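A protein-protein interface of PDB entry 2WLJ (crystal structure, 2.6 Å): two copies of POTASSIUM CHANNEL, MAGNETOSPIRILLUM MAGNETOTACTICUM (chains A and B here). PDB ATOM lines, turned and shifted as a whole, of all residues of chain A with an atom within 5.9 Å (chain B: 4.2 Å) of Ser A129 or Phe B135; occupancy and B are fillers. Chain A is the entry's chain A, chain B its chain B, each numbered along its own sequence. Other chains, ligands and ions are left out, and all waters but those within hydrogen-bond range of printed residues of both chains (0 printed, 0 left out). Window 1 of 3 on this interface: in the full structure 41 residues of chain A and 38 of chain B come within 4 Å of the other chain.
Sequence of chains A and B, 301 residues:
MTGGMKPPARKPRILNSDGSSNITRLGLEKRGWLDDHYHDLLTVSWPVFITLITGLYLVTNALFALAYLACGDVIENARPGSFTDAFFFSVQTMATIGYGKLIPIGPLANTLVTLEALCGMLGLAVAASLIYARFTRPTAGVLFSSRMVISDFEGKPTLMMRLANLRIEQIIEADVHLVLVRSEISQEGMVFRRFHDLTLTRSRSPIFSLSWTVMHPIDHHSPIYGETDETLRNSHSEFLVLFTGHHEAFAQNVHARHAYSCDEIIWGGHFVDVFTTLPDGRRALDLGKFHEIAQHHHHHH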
ATOM      1  N   TYR A  38      21.332 -16.416   0.369  1.00  0.00           N
ATOM      2  CA  TYR A  38      19.873 -16.468   0.536  1.00  0.00           C
ATOM      3  C   TYR A  38      19.331 -17.893   0.367  1.00  0.00           C
ATOM      4  O   TYR A  38      18.865 -18.504   1.340  1.00  0.00           O
ATOM      5  CB  TYR A  38      19.137 -15.504  -0.409  1.00  0.00           C
ATOM      6  CG  TYR A  38      17.629 -15.727  -0.413  1.00  0.00           C
ATOM      7  CD1 TYR A  38      16.884 -15.605   0.761  1.00  0.00           C
ATOM      8  CD2 TYR A  38      16.951 -16.078  -1.589  1.00  0.00           C
ATOM      9  CE1 TYR A  38      15.501 -15.821   0.765  1.00  0.00           C
ATOM     10  CE2 TYR A  38      15.567 -16.294  -1.594  1.00  0.00           C
ATOM     11  CZ  TYR A  38      14.853 -16.164  -0.413  1.00  0.00           C
ATOM     12  OH  TYR A  38      13.490 -16.370  -0.402  1.00  0.00           O
ATOM     13  N   LEU A 124      14.450  -8.673  12.307  1.00  0.00           N
ATOM     14  CA  LEU A 124      13.391  -9.568  12.775  1.00  0.00           C
ATOM     15  C   LEU A 124      12.537 -10.081  11.620  1.00  0.00           C
ATOM     16  O   LEU A 124      12.237 -11.278  11.520  1.00  0.00           O
ATOM     17  CB  LEU A 124      12.490  -8.863  13.789  1.00  0.00           C
ATOM     18  CG  LEU A 124      11.267  -9.660  14.233  1.00  0.00           C
ATOM     19  CD1 LEU A 124      11.705 -10.991  14.825  1.00  0.00           C
ATOM     20  CD2 LEU A 124      10.473  -8.871  15.274  1.00  0.00           C
ATOM     21  N   ALA A 125      12.163  -9.158  10.745  1.00  0.00           N
ATOM     22  CA  ALA A 125      11.239  -9.454   9.675  1.00  0.00           C
ATOM     23  C   ALA A 125      11.889 -10.449   8.762  1.00  0.00           C
ATOM     24  O   ALA A 125      11.261 -11.439   8.373  1.00  0.00           O
ATOM     25  CB  ALA A 125      10.907  -8.182   8.905  1.00  0.00           C
ATOM     26  N   VAL A 126      13.150 -10.190   8.412  1.00  0.00           N
ATOM     27  CA  VAL A 126      13.855 -11.091   7.524  1.00  0.00           C
ATOM     28  C   VAL A 126      13.968 -12.443   8.216  1.00  0.00           C
ATOM     29  O   VAL A 126      13.604 -13.472   7.658  1.00  0.00           O
ATOM     30  CB  VAL A 126      15.240 -10.572   7.104  1.00  0.00           C
ATOM     31  CG1 VAL A 126      15.978 -11.647   6.338  1.00  0.00           C
ATOM     32  CG2 VAL A 126      15.116  -9.340   6.223  1.00  0.00           C
ATOM     33  N   ALA A 127      14.412 -12.461   9.458  1.00  0.00           N
ATOM     34  CA  ALA A 127      14.560 -13.748  10.121  1.00  0.00           C
ATOM     35  C   ALA A 127      13.230 -14.485  10.208  1.00  0.00           C
ATOM     36  O   ALA A 127      13.193 -15.713  10.111  1.00  0.00           O
ATOM     37  CB  ALA A 127      15.177 -13.580  11.498  1.00  0.00           C
ATOM     38  N   ALA A 128      12.134 -13.759  10.395  1.00  0.00           N
ATOM     39  CA  ALA A 128      10.840 -14.422  10.420  1.00  0.00           C
ATOM     40  C   ALA A 128      10.481 -14.967   9.029  1.00  0.00           C
ATOM     41  O   ALA A 128       9.862 -16.024   8.897  1.00  0.00           O
ATOM     42  CB  ALA A 128       9.777 -13.479  10.919  1.00  0.00           C
ATOM     43  N   SER A 129      10.856 -14.241   7.988  1.00  0.00           N
ATOM     44  CA  SER A 129      10.649 -14.735   6.627  1.00  0.00           C
ATOM     45  C   SER A 129      11.379 -16.040   6.440  1.00  0.00           C
ATOM     46  O   SER A 129      10.805 -17.051   6.044  1.00  0.00           O
ATOM     47  CB  SER A 129      11.160 -13.729   5.609  1.00  0.00           C
ATOM     48  OG  SER A 129      10.326 -12.571   5.648  1.00  0.00           O
ATOM     49  N   LEU A 130      12.665 -16.030   6.722  1.00  0.00           N
ATOM     50  CA  LEU A 130      13.424 -17.227   6.460  1.00  0.00           C
ATOM     51  C   LEU A 130      12.853 -18.401   7.243  1.00  0.00           C
ATOM     52  O   LEU A 130      12.755 -19.514   6.742  1.00  0.00           O
ATOM     53  CB  LEU A 130      14.892 -16.978   6.772  1.00  0.00           C
ATOM     54  CG  LEU A 130      15.487 -15.911   5.836  1.00  0.00           C
ATOM     55  CD1 LEU A 130      16.906 -15.529   6.280  1.00  0.00           C
ATOM     56  CD2 LEU A 130      15.476 -16.376   4.364  1.00  0.00           C
ATOM     57  N   ILE A 131      12.441 -18.165   8.473  1.00  0.00           N
ATOM     58  CA  ILE A 131      11.949 -19.281   9.249  1.00  0.00           C
ATOM     59  C   ILE A 131      10.665 -19.859   8.650  1.00  0.00           C
ATOM     60  O   ILE A 131      10.505 -21.086   8.522  1.00  0.00           O
ATOM     61  CB  ILE A 131      11.717 -18.861  10.668  1.00  0.00           C
ATOM     62  CG1 ILE A 131      13.088 -18.664  11.348  1.00  0.00           C
ATOM     63  CG2 ILE A 131      10.850 -19.873  11.385  1.00  0.00           C
ATOM     64  CD1 ILE A 131      13.000 -18.168  12.772  1.00  0.00           C
ATOM     65  N   TYR A 132       9.747 -18.975   8.275  1.00  0.00           N
ATOM     66  CA  TYR A 132       8.524 -19.440   7.669  1.00  0.00           C
ATOM     67  C   TYR A 132       8.791 -20.175   6.339  1.00  0.00           C
ATOM     68  O   TYR A 132       8.234 -21.252   6.086  1.00  0.00           O
ATOM     69  CB  TYR A 132       7.530 -18.296   7.471  1.00  0.00           C
ATOM     70  CG  TYR A 132       6.251 -18.784   6.823  1.00  0.00           C
ATOM     71  CD1 TYR A 132       5.203 -19.270   7.586  1.00  0.00           C
ATOM     72  CD2 TYR A 132       6.115 -18.814   5.448  1.00  0.00           C
ATOM     73  CE1 TYR A 132       4.047 -19.749   6.999  1.00  0.00           C
ATOM     74  CE2 TYR A 132       4.961 -19.293   4.852  1.00  0.00           C
ATOM     75  CZ  TYR A 132       3.931 -19.749   5.644  1.00  0.00           C
ATOM     76  OH  TYR A 132       2.778 -20.207   5.060  1.00  0.00           O
ATOM     77  N   ALA A 133       9.654 -19.604   5.497  1.00  0.00           N
ATOM     78  CA  ALA A 133      10.009 -20.228   4.228  1.00  0.00           C
ATOM     79  C   ALA A 133      10.547 -21.637   4.435  1.00  0.00           C
ATOM     80  O   ALA A 133      10.218 -22.548   3.706  1.00  0.00           O
ATOM     81  CB  ALA A 133      11.016 -19.384   3.489  1.00  0.00           C
ATOM     82  N   ARG A 134      11.394 -21.814   5.428  1.00  0.00           N
ATOM     83  CA  ARG A 134      11.967 -23.114   5.676  1.00  0.00           C
ATOM     84  C   ARG A 134      10.877 -24.067   6.093  1.00  0.00           C
ATOM     85  O   ARG A 134      10.902 -25.233   5.719  1.00  0.00           O
ATOM     86  CB  ARG A 134      13.074 -23.022   6.721  1.00  0.00           C
ATOM     87  CG  ARG A 134      14.314 -22.309   6.172  1.00  0.00           C
ATOM     88  CD  ARG A 134      15.287 -21.894   7.275  1.00  0.00           C
ATOM     89  NE  ARG A 134      15.647 -23.035   8.102  1.00  0.00           N
ATOM     90  CZ  ARG A 134      16.588 -23.918   7.781  1.00  0.00           C
ATOM     91  NH1 ARG A 134      17.290 -23.796   6.654  1.00  0.00           N
ATOM     92  NH2 ARG A 134      16.829 -24.923   8.604  1.00  0.00           N
ATOM     93  N   TRP B  46      16.144  -3.907  -4.118  1.00  0.00           N
ATOM     94  CA  TRP B  46      16.271  -3.924  -2.679  1.00  0.00           C
ATOM     95  C   TRP B  46      16.743  -2.577  -2.106  1.00  0.00           C
ATOM     96  O   TRP B  46      16.043  -1.981  -1.266  1.00  0.00           O
ATOM     97  CB  TRP B  46      17.094  -5.120  -2.197  1.00  0.00           C
ATOM     98  CG  TRP B  46      16.265  -6.375  -2.164  1.00  0.00           C
ATOM     99  CD1 TRP B  46      16.265  -7.375  -3.086  1.00  0.00           C
ATOM    100  CD2 TRP B  46      15.278  -6.747  -1.176  1.00  0.00           C
ATOM    101  NE1 TRP B  46      15.361  -8.354  -2.731  1.00  0.00           N
ATOM    102  CE2 TRP B  46      14.747  -7.995  -1.564  1.00  0.00           C
ATOM    103  CE3 TRP B  46      14.806  -6.153   0.000  1.00  0.00           C
ATOM    104  CZ2 TRP B  46      13.764  -8.651  -0.828  1.00  0.00           C
ATOM    105  CZ3 TRP B  46      13.832  -6.816   0.741  1.00  0.00           C
ATOM    106  CH2 TRP B  46      13.321  -8.048   0.319  1.00  0.00           C
ATOM    107  N   ILE B 131       8.487  -7.570   2.688  1.00  0.00           N
ATOM    108  CA  ILE B 131       9.703  -8.355   2.537  1.00  0.00           C
ATOM    109  C   ILE B 131       9.406  -9.845   2.249  1.00  0.00           C
ATOM    110  O   ILE B 131       9.968 -10.459   1.313  1.00  0.00           O
ATOM    111  CB  ILE B 131      10.501  -8.286   3.802  1.00  0.00           C
ATOM    112  CG1 ILE B 131      11.194  -6.936   3.874  1.00  0.00           C
ATOM    113  CG2 ILE B 131      11.479  -9.394   3.855  1.00  0.00           C
ATOM    114  CD1 ILE B 131      11.586  -6.549   5.264  1.00  0.00           C
ATOM    115  N   TYR B 132       8.534 -10.444   3.054  1.00  0.00           N
ATOM    116  CA  TYR B 132       8.243 -11.820   2.789  1.00  0.00           C
ATOM    117  C   TYR B 132       7.731 -11.977   1.345  1.00  0.00           C
ATOM    118  O   TYR B 132       8.093 -12.935   0.643  1.00  0.00           O
ATOM    119  CB  TYR B 132       7.267 -12.440   3.787  1.00  0.00           C
ATOM    120  CG  TYR B 132       7.053 -13.886   3.401  1.00  0.00           C
ATOM    121  CD1 TYR B 132       8.062 -14.829   3.579  1.00  0.00           C
ATOM    122  CD2 TYR B 132       5.899 -14.288   2.769  1.00  0.00           C
ATOM    123  CE1 TYR B 132       7.905 -16.142   3.176  1.00  0.00           C
ATOM    124  CE2 TYR B 132       5.715 -15.601   2.374  1.00  0.00           C
ATOM    125  CZ  TYR B 132       6.725 -16.519   2.582  1.00  0.00           C
ATOM    126  OH  TYR B 132       6.536 -17.815   2.174  1.00  0.00           O
ATOM    127  N   ALA B 133       6.891 -11.041   0.902  1.00  0.00           N
ATOM    128  CA  ALA B 133       6.298 -11.141  -0.415  1.00  0.00           C
ATOM    129  C   ALA B 133       7.415 -11.062  -1.406  1.00  0.00           C
ATOM    130  O   ALA B 133       7.560 -11.942  -2.238  1.00  0.00           O
ATOM    131  CB  ALA B 133       5.314 -10.033  -0.665  1.00  0.00           C
ATOM    132  N   ARG B 134       8.211 -10.004  -1.313  1.00  0.00           N
ATOM    133  CA  ARG B 134       9.246  -9.763  -2.298  1.00  0.00           C
ATOM    134  C   ARG B 134      10.108 -11.003  -2.467  1.00  0.00           C
ATOM    135  O   ARG B 134      10.590 -11.281  -3.558  1.00  0.00           O
ATOM    136  CB  ARG B 134      10.085  -8.551  -1.916  1.00  0.00           C
ATOM    137  CG  ARG B 134       9.456  -7.223  -2.330  1.00  0.00           C
ATOM    138  CD  ARG B 134      10.150  -6.011  -1.645  1.00  0.00           C
ATOM    139  NE  ARG B 134      11.565  -5.923  -2.002  1.00  0.00           N
ATOM    140  CZ  ARG B 134      12.033  -5.313  -3.096  1.00  0.00           C
ATOM    141  NH1 ARG B 134      11.210  -4.705  -3.946  1.00  0.00           N
ATOM    142  NH2 ARG B 134      13.334  -5.301  -3.328  1.00  0.00           N
ATOM    143  N   PHE B 135      10.258 -11.756  -1.384  1.00  0.00           N
ATOM    144  CA  PHE B 135      11.033 -12.993  -1.356  1.00  0.00           C
ATOM    145  C   PHE B 135      10.359 -14.108  -2.140  1.00  0.00           C
ATOM    146  O   PHE B 135      10.977 -15.129  -2.434  1.00  0.00           O
ATOM    147  CB  PHE B 135      11.162 -13.493   0.069  1.00  0.00           C
ATOM    148  CG  PHE B 135      12.317 -12.921   0.810  1.00  0.00           C
ATOM    149  CD1 PHE B 135      12.930 -11.772   0.379  1.00  0.00           C
ATOM    150  CD2 PHE B 135      12.762 -13.518   1.980  1.00  0.00           C
ATOM    151  CE1 PHE B 135      14.002 -11.233   1.088  1.00  0.00           C
ATOM    152  CE2 PHE B 135      13.815 -12.987   2.696  1.00  0.00           C
ATOM    153  CZ  PHE B 135      14.443 -11.843   2.247  1.00  0.00           C
ATOM    154  N   THR B 136       9.085 -13.925  -2.451  1.00  0.00           N
ATOM    155  CA  THR B 136       8.321 -15.000  -3.038  1.00  0.00           C
ATOM    156  C   THR B 136       7.700 -14.618  -4.369  1.00  0.00           C
ATOM    157  O   THR B 136       6.759 -15.273  -4.819  1.00  0.00           O
ATOM    158  CB  THR B 136       7.230 -15.538  -2.070  1.00  0.00           C
ATOM    159  OG1 THR B 136       6.216 -14.540  -1.863  1.00  0.00           O
ATOM    160  CG2 THR B 136       7.855 -15.948  -0.734  1.00  0.00           C
ATOM    161  N   ARG B 137       8.210 -13.564  -4.999  1.00  0.00           N
ATOM    162  CA  ARG B 137       7.900 -13.343  -6.402  1.00  0.00           C
ATOM    163  C   ARG B 137       9.189 -13.447  -7.234  1.00  0.00           C
ATOM    164  O   ARG B 137       9.622 -12.468  -7.869  1.00  0.00           O
ATOM    165  CB  ARG B 137       7.183 -12.015  -6.641  1.00  0.00           C
ATOM    166  CG  ARG B 137       8.089 -10.797  -6.717  1.00  0.00           C
ATOM    167  CD  ARG B 137       7.430  -9.593  -7.432  1.00  0.00           C
ATOM    168  NE  ARG B 137       6.000  -9.442  -7.130  1.00  0.00           N
ATOM    169  CZ  ARG B 137       5.183  -8.564  -7.723  1.00  0.00           C
ATOM    170  NH1 ARG B 137       5.649  -7.733  -8.652  1.00  0.00           N
ATOM    171  NH2 ARG B 137       3.894  -8.512  -7.387  1.00  0.00           N
ATOM    172  N   GLN B 252       8.031 -22.427  -5.504  1.00  0.00           N
ATOM    173  CA  GLN B 252       6.860 -21.701  -5.997  1.00  0.00           C
ATOM    174  C   GLN B 252       6.961 -21.731  -7.529  1.00  0.00           C
ATOM    175  O   GLN B 252       8.070 -21.832  -8.082  1.00  0.00           O
ATOM    176  CB  GLN B 252       6.866 -20.248  -5.528  1.00  0.00           C
ATOM    177  CG  GLN B 252       7.654 -19.993  -4.263  1.00  0.00           C
ATOM    178  CD  GLN B 252       8.134 -18.554  -4.168  1.00  0.00           C
ATOM    179  OE1 GLN B 252       8.955 -18.218  -3.309  1.00  0.00           O
ATOM    180  NE2 GLN B 252       7.626 -17.695  -5.059  1.00  0.00           N
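O of Phe B135 sits at hydrogen-bond distance from OH of Tyr A38 (3.5 Å).
O of Ala A125 sits at hydrogen-bond distance from OG of Ser A129 (3.1 Å).
OG of Ser A129 touches CG2 of Ile B131 (3.8 Å). Ser A129 touches Tyr B132 (OG to CB, 3.6 Å). Phe B135 touches Ser A129 (CD2 to CB, 3.97 Å). Tyr A132 touches Tyr B132 (CE2 to OH, 3.4 Å).
Printed residues of chain B within 4 Å of Tyr A38: Phe B135. Ser A129 touches just these residues of chain B: Ile B131, Tyr B132 and Phe B135. Of the printed residues of chain B, Tyr A132 touches Tyr B132 (3.4 Å). Printed residues of chain A within 4 Å of Ile B131: Ser A129. Printed residues of chain A within 4 Å of Tyr B132: Ser A129 and Tyr A132. Ala B133 touches none of the printed residues of chain A. Of the printed residues of chain A, Phe B135 touches Tyr A38 and Ser A129. The nearest printed residue of chain B that does not touch Ser A129 is Ala B133 (6.1 Å).
Of the 12 printed residues of chain A, 3 touch a printed residue of chain B. Hydrophobic or aromatic side chains of chain B within 4 Å of the printed part of chain A: Ile B131, Tyr B132 and Phe B135. Among the printed residues, 5 pairs touch across the chains. Among the printed residues, no Asp or Glu carboxylate lies within 4 Å of a Lys or Arg side-chain nitrogen of the other chain.
Tyr A132 touches its own counterpart, Tyr B132. 4 positions are printed for both chains. Of the 5 pairs that touch across the chains among the printed residues, 1 has its exchanged pair printed and touching as well.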
